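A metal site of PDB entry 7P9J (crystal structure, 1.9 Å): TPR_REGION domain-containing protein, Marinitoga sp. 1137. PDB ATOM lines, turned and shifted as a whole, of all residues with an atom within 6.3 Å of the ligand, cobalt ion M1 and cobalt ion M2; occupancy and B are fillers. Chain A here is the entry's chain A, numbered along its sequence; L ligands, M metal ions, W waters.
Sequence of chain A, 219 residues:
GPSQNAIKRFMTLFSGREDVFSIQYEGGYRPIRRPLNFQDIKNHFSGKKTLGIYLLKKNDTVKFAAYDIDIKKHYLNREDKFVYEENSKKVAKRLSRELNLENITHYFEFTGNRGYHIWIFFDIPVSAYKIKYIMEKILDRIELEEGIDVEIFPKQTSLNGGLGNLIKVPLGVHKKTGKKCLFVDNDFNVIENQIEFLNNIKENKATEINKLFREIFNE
Of the 21 residues printed, 3 come within 4 Å of cobalt ion M1. The nearest printed residue that does not touch cobalt ion M1 is Arg 114 (4.4 Å).
Tyr 29 touches the ligand. N of Gly 115 touches O6 of the ligand (3.6 Å). CZ of Phe 153 touches O10 of the ligand, at 3.6 Å. Leu 166 touches the ligand. CA of Ile 167 touches O7 of the ligand, 3.7 Å away. Of the 21 residues printed, 13 come within 4 Å of the ligand.
OD1 of Asp 68 lies close to NE2 of His 117 (3.3 Å). The side-chain carboxylate (OD2) of Asp 70 lies close to the guanidinium group (NE) of Arg 114 (3.2 Å). O of Thr 111 lies within hydrogen-bond range of NZ of Lys 168 (3.1 Å). The side-chain hydroxyl (OG1) of Thr 111 lies within hydrogen-bond range of the backbone carbonyl oxygen (O) of Gly 115 (2.8 Å).
OE2 of Glu 151 binds cobalt ion M1, at 1.9 Å. Cobalt ion M1 is bound by OD2 of Asp 68 (2.2 Å). Cobalt ion M1 is bound by O1 of the ligand, at 2.5 Å. Cobalt ion M1 is bound by OD2 of Asp 70, 2.5 Å away. Cobalt ion M1 has four donor atoms within binding distance.
Cobalt ion M2 is bound by O1 of the ligand (2.0 Å), water W5 (2.0 Å), O5 of the ligand (2.2 Å), O3 of the ligand (2.2 Å), OD1 of Asp 70 (2.2 Å) and OD1 of Asp 68 (2.5 Å). Cobalt ion M2 has six donor atoms within binding distance.
The side-chain hydroxyl (OG1) of Thr 111 lies within hydrogen-bond range of an oxygen (O6) of the ligand (2.6 Å). The backbone NH of Lys 168 is in hydrogen-bond range of an oxygen (O7) of the ligand (2.8 Å). The side-chain amino group of Lys 168 lies within salt-bridge range of an oxygen (O2) of the ligand, at 3.3 Å. NE2 of His 117 sits close to O2 of the ligand, 3.5 Å away. The backbone NH of Arg 114 sits at hydrogen-bond distance from an oxygen (O6) of the ligand, at 2.9 Å. An oxygen (O4) of the ligand is in salt-bridge range of the guanidinium group of Arg 114. O9 of the ligand is in hydrogen-bond range of NE2 of His 174 (3.0 Å). The side-chain amide nitrogen of Asn 113 sits at hydrogen-bond distance from an oxygen (O9) of the ligand, at 3.1 Å.
Merely in contact with cobalt ion M2: Arg 114 (3.99 Å). Three residues have an atom within 4 Å of cobalt ion M2: Asp 68, Asp 70 and Arg 114. Along chain A the residues within 4 Å of cobalt ion M2 span positions 68 to 114. The nearest printed residue that does not touch cobalt ion M2 is His 117 (4.3 Å).
Water W1 lies within hydrogen-bond range of an oxygen (O9) of the ligand and the guanidinium group of Arg 114. Water W2 lies within hydrogen-bond range of OH of Tyr 29 (3.1 Å) and N6 of the ligand (3.3 Å).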
ATOM      1  N   GLY A  27      33.938 -10.150  23.385  1.00  0.00           N
ATOM      2  CA  GLY A  27      34.719 -10.995  22.506  1.00  0.00           C
ATOM      3  C   GLY A  27      35.287 -12.267  23.117  1.00  0.00           C
ATOM      4  O   GLY A  27      36.177 -12.876  22.517  1.00  0.00           O
ATOM      5  N   GLY A  28      34.746 -12.689  24.261  1.00  0.00           N
ATOM      6  CA  GLY A  28      35.157 -13.971  24.835  1.00  0.00           C
ATOM      7  C   GLY A  28      35.028 -14.047  26.337  1.00  0.00           C
ATOM      8  O   GLY A  28      34.384 -13.169  26.917  1.00  0.00           O
ATOM      9  N   TYR A  29      35.595 -15.098  26.919  1.00  0.00           N
ATOM     10  CA  TYR A  29      35.587 -15.251  28.387  1.00  0.00           C
ATOM     11  C   TYR A  29      37.040 -15.283  28.859  1.00  0.00           C
ATOM     12  O   TYR A  29      37.877 -15.887  28.181  1.00  0.00           O
ATOM     13  CB  TYR A  29      34.784 -16.492  28.785  1.00  0.00           C
ATOM     14  CG  TYR A  29      33.299 -16.371  28.656  1.00  0.00           C
ATOM     15  CD1 TYR A  29      32.683 -16.431  27.418  1.00  0.00           C
ATOM     16  CD2 TYR A  29      32.486 -16.214  29.763  1.00  0.00           C
ATOM     17  CE1 TYR A  29      31.304 -16.321  27.281  1.00  0.00           C
ATOM     18  CE2 TYR A  29      31.113 -16.116  29.653  1.00  0.00           C
ATOM     19  CZ  TYR A  29      30.525 -16.166  28.410  1.00  0.00           C
ATOM     20  OH  TYR A  29      29.167 -16.065  28.277  1.00  0.00           O
ATOM     21  N   GLY A  52      31.356 -16.943  33.916  1.00  0.00           N
ATOM     22  CA  GLY A  52      31.332 -18.244  33.276  1.00  0.00           C
ATOM     23  C   GLY A  52      32.040 -19.282  34.133  1.00  0.00           C
ATOM     24  O   GLY A  52      33.211 -19.092  34.492  1.00  0.00           O
ATOM     25  N   ASP A  68      21.770 -26.433  26.362  1.00  0.00           N
ATOM     26  CA  ASP A  68      21.779 -25.100  25.750  1.00  0.00           C
ATOM     27  C   ASP A  68      20.947 -25.123  24.477  1.00  0.00           C
ATOM     28  O   ASP A  68      21.350 -25.754  23.490  1.00  0.00           O
ATOM     29  CB  ASP A  68      23.208 -24.675  25.451  1.00  0.00           C
ATOM     30  CG  ASP A  68      23.295 -23.287  24.847  1.00  0.00           C
ATOM     31  OD1 ASP A  68      22.391 -22.441  25.020  1.00  0.00           O
ATOM     32  OD2 ASP A  68      24.306 -23.096  24.143  1.00  0.00           O
ATOM     33  N   ILE A  69      19.794 -24.445  24.486  1.00  0.00           N
ATOM     34  CA  ILE A  69      18.925 -24.386  23.320  1.00  0.00           C
ATOM     35  C   ILE A  69      19.089 -23.035  22.633  1.00  0.00           C
ATOM     36  O   ILE A  69      18.835 -21.981  23.242  1.00  0.00           O
ATOM     37  CB  ILE A  69      17.455 -24.646  23.701  1.00  0.00           C
ATOM     38  CG1 ILE A  69      17.313 -25.966  24.483  1.00  0.00           C
ATOM     39  CG2 ILE A  69      16.616 -24.720  22.450  1.00  0.00           C
ATOM     40  CD1 ILE A  69      17.087 -25.793  25.956  1.00  0.00           C
ATOM     41  N   ASP A  70      19.475 -23.061  21.356  1.00  0.00           N
ATOM     42  CA  ASP A  70      19.892 -21.879  20.607  1.00  0.00           C
ATOM     43  C   ASP A  70      19.106 -21.761  19.317  1.00  0.00           C
ATOM     44  O   ASP A  70      18.935 -22.760  18.614  1.00  0.00           O
ATOM     45  CB  ASP A  70      21.375 -21.948  20.171  1.00  0.00           C
ATOM     46  CG  ASP A  70      22.309 -21.545  21.258  1.00  0.00           C
ATOM     47  OD1 ASP A  70      21.834 -21.186  22.329  1.00  0.00           O
ATOM     48  OD2 ASP A  70      23.525 -21.583  21.008  1.00  0.00           O
ATOM     49  N   THR A 111      18.522 -16.968  28.479  1.00  0.00           N
ATOM     50  CA  THR A 111      19.968 -16.645  28.365  1.00  0.00           C
ATOM     51  C   THR A 111      20.296 -15.172  28.070  1.00  0.00           C
ATOM     52  O   THR A 111      21.481 -14.856  28.039  1.00  0.00           O
ATOM     53  CB  THR A 111      20.593 -17.537  27.292  1.00  0.00           C
ATOM     54  OG1 THR A 111      19.931 -17.319  26.055  1.00  0.00           O
ATOM     55  CG2 THR A 111      20.513 -19.001  27.667  1.00  0.00           C
ATOM     56  N   GLY A 112      19.306 -14.334  27.835  1.00  0.00           N
ATOM     57  CA  GLY A 112      19.576 -12.899  27.632  1.00  0.00           C
ATOM     58  C   GLY A 112      19.907 -12.541  26.203  1.00  0.00           C
ATOM     59  O   GLY A 112      20.312 -11.409  25.986  1.00  0.00           O
ATOM     60  N   ASN A 113      19.718 -13.461  25.261  1.00  0.00           N
ATOM     61  CA  ASN A 113      19.996 -13.191  23.826  1.00  0.00           C
ATOM     62  C   ASN A 113      19.171 -14.068  22.896  1.00  0.00           C
ATOM     63  O   ASN A 113      18.190 -13.556  22.354  1.00  0.00           O
ATOM     64  CB  ASN A 113      21.486 -13.351  23.483  1.00  0.00           C
ATOM     65  CG  ASN A 113      21.817 -13.116  22.019  1.00  0.00           C
ATOM     66  OD1 ASN A 113      21.222 -12.271  21.362  1.00  0.00           O
ATOM     67  ND2 ASN A 113      22.773 -13.865  21.510  1.00  0.00           N
ATOM     68  N   ARG A 114      19.547 -15.344  22.728  1.00  0.00           N
ATOM     69  CA  ARG A 114      18.873 -16.175  21.700  1.00  0.00           C
ATOM     70  C   ARG A 114      18.361 -17.513  22.234  1.00  0.00           C
ATOM     71  O   ARG A 114      18.088 -18.390  21.405  1.00  0.00           O
ATOM     72  CB  ARG A 114      19.837 -16.457  20.546  1.00  0.00           C
ATOM     73  CG  ARG A 114      21.231 -16.896  20.954  1.00  0.00           C
ATOM     74  CD  ARG A 114      21.658 -18.110  20.172  1.00  0.00           C
ATOM     75  NE  ARG A 114      23.039 -18.471  20.394  1.00  0.00           N
ATOM     76  CZ  ARG A 114      23.934 -18.676  19.437  1.00  0.00           C
ATOM     77  NH1 ARG A 114      23.588 -18.562  18.164  1.00  0.00           N
ATOM     78  NH2 ARG A 114      25.173 -19.007  19.757  1.00  0.00           N
ATOM     79  N   GLY A 115      18.235 -17.682  23.536  1.00  0.00           N
ATOM     80  CA  GLY A 115      17.709 -19.002  23.910  1.00  0.00           C
ATOM     81  C   GLY A 115      17.533 -19.313  25.372  1.00  0.00           C
ATOM     82  O   GLY A 115      17.344 -18.377  26.160  1.00  0.00           O
ATOM     83  N   TYR A 116      17.583 -20.598  25.680  1.00  0.00           N
ATOM     84  CA  TYR A 116      17.281 -21.038  27.057  1.00  0.00           C
ATOM     85  C   TYR A 116      18.311 -22.050  27.551  1.00  0.00           C
ATOM     86  O   TYR A 116      18.865 -22.800  26.732  1.00  0.00           O
ATOM     87  CB  TYR A 116      15.878 -21.640  27.039  1.00  0.00           C
ATOM     88  CG  TYR A 116      14.763 -20.647  26.837  1.00  0.00           C
ATOM     89  CD1 TYR A 116      14.319 -19.858  27.888  1.00  0.00           C
ATOM     90  CD2 TYR A 116      14.165 -20.484  25.601  1.00  0.00           C
ATOM     91  CE1 TYR A 116      13.301 -18.936  27.715  1.00  0.00           C
ATOM     92  CE2 TYR A 116      13.157 -19.546  25.411  1.00  0.00           C
ATOM     93  CZ  TYR A 116      12.724 -18.785  26.473  1.00  0.00           C
ATOM     94  OH  TYR A 116      11.720 -17.872  26.282  1.00  0.00           O
ATOM     95  N   HIS A 117      18.562 -22.053  28.853  1.00  0.00           N
ATOM     96  CA  HIS A 117      19.429 -23.096  29.439  1.00  0.00           C
ATOM     97  C   HIS A 117      18.526 -23.937  30.342  1.00  0.00           C
ATOM     98  O   HIS A 117      17.692 -23.362  31.043  1.00  0.00           O
ATOM     99  CB  HIS A 117      20.573 -22.500  30.267  1.00  0.00           C
ATOM    100  CG  HIS A 117      21.695 -21.926  29.496  1.00  0.00           C
ATOM    101  ND1 HIS A 117      22.523 -20.967  30.022  1.00  0.00           N
ATOM    102  CD2 HIS A 117      22.147 -22.173  28.247  1.00  0.00           C
ATOM    103  CE1 HIS A 117      23.435 -20.644  29.144  1.00  0.00           C
ATOM    104  NE2 HIS A 117      23.233 -21.364  28.051  1.00  0.00           N
ATOM    105  N   GLU A 151      22.791 -28.054  22.462  1.00  0.00           N
ATOM    106  CA  GLU A 151      24.113 -28.416  22.936  1.00  0.00           C
ATOM    107  C   GLU A 151      24.014 -28.855  24.396  1.00  0.00           C
ATOM    108  O   GLU A 151      23.177 -28.348  25.137  1.00  0.00           O
ATOM    109  CB  GLU A 151      25.086 -27.241  22.726  1.00  0.00           C
ATOM    110  CG  GLU A 151      24.871 -26.542  21.343  1.00  0.00           C
ATOM    111  CD  GLU A 151      24.066 -25.220  21.334  1.00  0.00           C
ATOM    112  OE1 GLU A 151      22.823 -25.249  21.113  1.00  0.00           O
ATOM    113  OE2 GLU A 151      24.676 -24.127  21.436  1.00  0.00           O
ATOM    114  N   PHE A 153      26.068 -29.530  27.951  1.00  0.00           N
ATOM    115  CA  PHE A 153      27.218 -29.198  28.761  1.00  0.00           C
ATOM    116  C   PHE A 153      27.222 -30.105  29.974  1.00  0.00           C
ATOM    117  O   PHE A 153      26.188 -30.208  30.641  1.00  0.00           O
ATOM    118  CB  PHE A 153      27.154 -27.728  29.222  1.00  0.00           C
ATOM    119  CG  PHE A 153      27.594 -26.743  28.187  1.00  0.00           C
ATOM    120  CD1 PHE A 153      26.685 -26.212  27.277  1.00  0.00           C
ATOM    121  CD2 PHE A 153      28.914 -26.323  28.132  1.00  0.00           C
ATOM    122  CE1 PHE A 153      27.081 -25.270  26.327  1.00  0.00           C
ATOM    123  CE2 PHE A 153      29.324 -25.382  27.182  1.00  0.00           C
ATOM    124  CZ  PHE A 153      28.414 -24.865  26.277  1.00  0.00           C
ATOM    125  N   LEU A 166      33.059 -24.022  29.574  1.00  0.00           N
ATOM    126  CA  LEU A 166      32.533 -23.089  30.574  1.00  0.00           C
ATOM    127  C   LEU A 166      31.131 -22.679  30.114  1.00  0.00           C
ATOM    128  O   LEU A 166      30.841 -22.736  28.914  1.00  0.00           O
ATOM    129  CB  LEU A 166      33.469 -21.873  30.739  1.00  0.00           C
ATOM    130  CG  LEU A 166      33.605 -20.835  29.621  1.00  0.00           C
ATOM    131  CD1 LEU A 166      32.507 -19.746  29.649  1.00  0.00           C
ATOM    132  CD2 LEU A 166      34.991 -20.214  29.587  1.00  0.00           C
ATOM    133  N   ILE A 167      30.272 -22.298  31.061  1.00  0.00           N
ATOM    134  CA  ILE A 167      28.912 -21.859  30.719  1.00  0.00           C
ATOM    135  C   ILE A 167      28.573 -20.614  31.529  1.00  0.00           C
ATOM    136  O   ILE A 167      28.942 -20.505  32.696  1.00  0.00           O
ATOM    137  CB  ILE A 167      27.865 -22.978  30.981  1.00  0.00           C
ATOM    138  CG1 ILE A 167      26.482 -22.512  30.551  1.00  0.00           C
ATOM    139  CG2 ILE A 167      27.824 -23.407  32.448  1.00  0.00           C
ATOM    140  CD1 ILE A 167      25.466 -23.607  30.445  1.00  0.00           C
ATOM    141  N   LYS A 168      27.861 -19.666  30.896  1.00  0.00           N
ATOM    142  CA  LYS A 168      27.383 -18.481  31.614  1.00  0.00           C
ATOM    143  C   LYS A 168      26.208 -18.851  32.516  1.00  0.00           C
ATOM    144  O   LYS A 168      25.246 -19.479  32.069  1.00  0.00           O
ATOM    145  CB  LYS A 168      26.952 -17.369  30.635  1.00  0.00           C
ATOM    146  CG  LYS A 168      26.295 -16.140  31.327  1.00  0.00           C
ATOM    147  CD  LYS A 168      26.188 -14.931  30.388  1.00  0.00           C
ATOM    148  CE  LYS A 168      25.581 -15.314  29.016  1.00  0.00           C
ATOM    149  NZ  LYS A 168      24.214 -15.937  29.104  1.00  0.00           N
ATOM    150  N   VAL A 169      26.277 -18.421  33.778  1.00  0.00           N
ATOM    151  CA  VAL A 169      25.338 -18.873  34.799  1.00  0.00           C
ATOM    152  C   VAL A 169      24.280 -17.799  35.040  1.00  0.00           C
ATOM    153  O   VAL A 169      24.545 -16.600  34.808  1.00  0.00           O
ATOM    154  CB  VAL A 169      26.093 -19.250  36.091  1.00  0.00           C
ATOM    155  CG1 VAL A 169      26.939 -20.487  35.857  1.00  0.00           C
ATOM    156  CG2 VAL A 169      26.918 -18.072  36.621  1.00  0.00           C
ATOM    157  N   HIS A 174      24.016 -10.654  30.159  1.00  0.00           N
ATOM    158  CA  HIS A 174      24.695 -11.084  28.931  1.00  0.00           C
ATOM    159  C   HIS A 174      25.420  -9.902  28.319  1.00  0.00           C
ATOM    160  O   HIS A 174      24.782  -8.929  27.891  1.00  0.00           O
ATOM    161  CB  HIS A 174      23.659 -11.649  27.957  1.00  0.00           C
ATOM    162  CG  HIS A 174      24.246 -12.503  26.889  1.00  0.00           C
ATOM    163  ND1 HIS A 174      25.510 -12.285  26.366  1.00  0.00           N
ATOM    164  CD2 HIS A 174      23.762 -13.601  26.255  1.00  0.00           C
ATOM    165  CE1 HIS A 174      25.762 -13.206  25.451  1.00  0.00           C
ATOM    166  NE2 HIS A 174      24.729 -14.019  25.366  1.00  0.00           N
HETATM  167  N1  LIG L   1      34.797 -18.632  24.860  1.00  0.00           N
HETATM  168  C1  LIG L   1      34.499 -19.451  25.876  1.00  0.00           C
HETATM  169  N2  LIG L   1      33.308 -19.943  26.254  1.00  0.00           N
HETATM  170  C2  LIG L   1      32.349 -19.504  25.460  1.00  0.00           C
HETATM  171  C3  LIG L   1      32.541 -18.643  24.362  1.00  0.00           C
HETATM  172  C4  LIG L   1      33.795 -18.239  24.107  1.00  0.00           C
HETATM  173  N3  LIG L   1      34.033 -17.361  22.991  1.00  0.00           N
HETATM  174  N4  LIG L   1      31.196 -18.406  23.735  1.00  0.00           N
HETATM  175  C5  LIG L   1      30.390 -19.131  24.523  1.00  0.00           C
HETATM  176  N5  LIG L   1      31.086 -19.703  25.432  1.00  0.00           N
HETATM  177  P1  LIG L   1      26.186 -19.688  23.697  1.00  0.00           P
HETATM  178  P2  LIG L   1      24.651 -18.532  25.932  1.00  0.00           P
HETATM  179  P3  LIG L   1      23.005 -17.094  24.178  1.00  0.00           P
HETATM  180  C6  LIG L   1      30.449 -20.511  26.404  1.00  0.00           C
HETATM  181  O1  LIG L   1      25.016 -20.378  23.257  1.00  0.00           O
HETATM  182  O2  LIG L   1      25.064 -18.529  27.317  1.00  0.00           O
HETATM  183  O3  LIG L   1      23.075 -18.271  23.352  1.00  0.00           O
HETATM  184  C7  LIG L   1      29.692 -19.614  27.391  1.00  0.00           C
HETATM  185  O4  LIG L   1      26.609 -19.089  22.458  1.00  0.00           O
HETATM  186  O5  LIG L   1      23.975 -19.774  25.808  1.00  0.00           O
HETATM  187  O6  LIG L   1      21.627 -16.716  24.122  1.00  0.00           O
HETATM  188  C8  LIG L   1      28.288 -19.851  27.033  1.00  0.00           C
HETATM  189  O7  LIG L   1      27.421 -19.720  28.152  1.00  0.00           O
HETATM  190  N6  LIG L   1      25.922 -18.438  24.831  1.00  0.00           N
HETATM  191  O8  LIG L   1      23.593 -17.324  25.671  1.00  0.00           O
HETATM  192  O9  LIG L   1      23.694 -16.076  23.441  1.00  0.00           O
HETATM  193  C9  LIG L   1      28.239 -21.222  26.477  1.00  0.00           C
HETATM  194  O10 LIG L   1      29.501 -21.470  25.859  1.00  0.00           O
HETATM  195  C10 LIG L   1      27.076 -21.365  25.488  1.00  0.00           C
HETATM  196  O11 LIG L   1      27.319 -20.713  24.282  1.00  0.00           O
HETATM  197 CO    CO M   1      25.393 -22.608  22.312  1.00  0.00          CO
HETATM  198 CO    CO M   2      23.160 -20.394  23.887  1.00  0.00          CO
HETATM  199  O   HOH W   1      25.613 -16.363  21.689  1.00  0.00           O
HETATM  200  O   HOH W   2      28.282 -16.214  25.352  1.00  0.00           O
HETATM  201  O   HOH W   3      31.016 -16.629  21.567  1.00  0.00           O
HETATM  202  O   HOH W   4      36.538 -18.379  21.923  1.00  0.00           O
HETATM  203  O   HOH W   5      21.288 -20.328  24.613  1.00  0.00           O
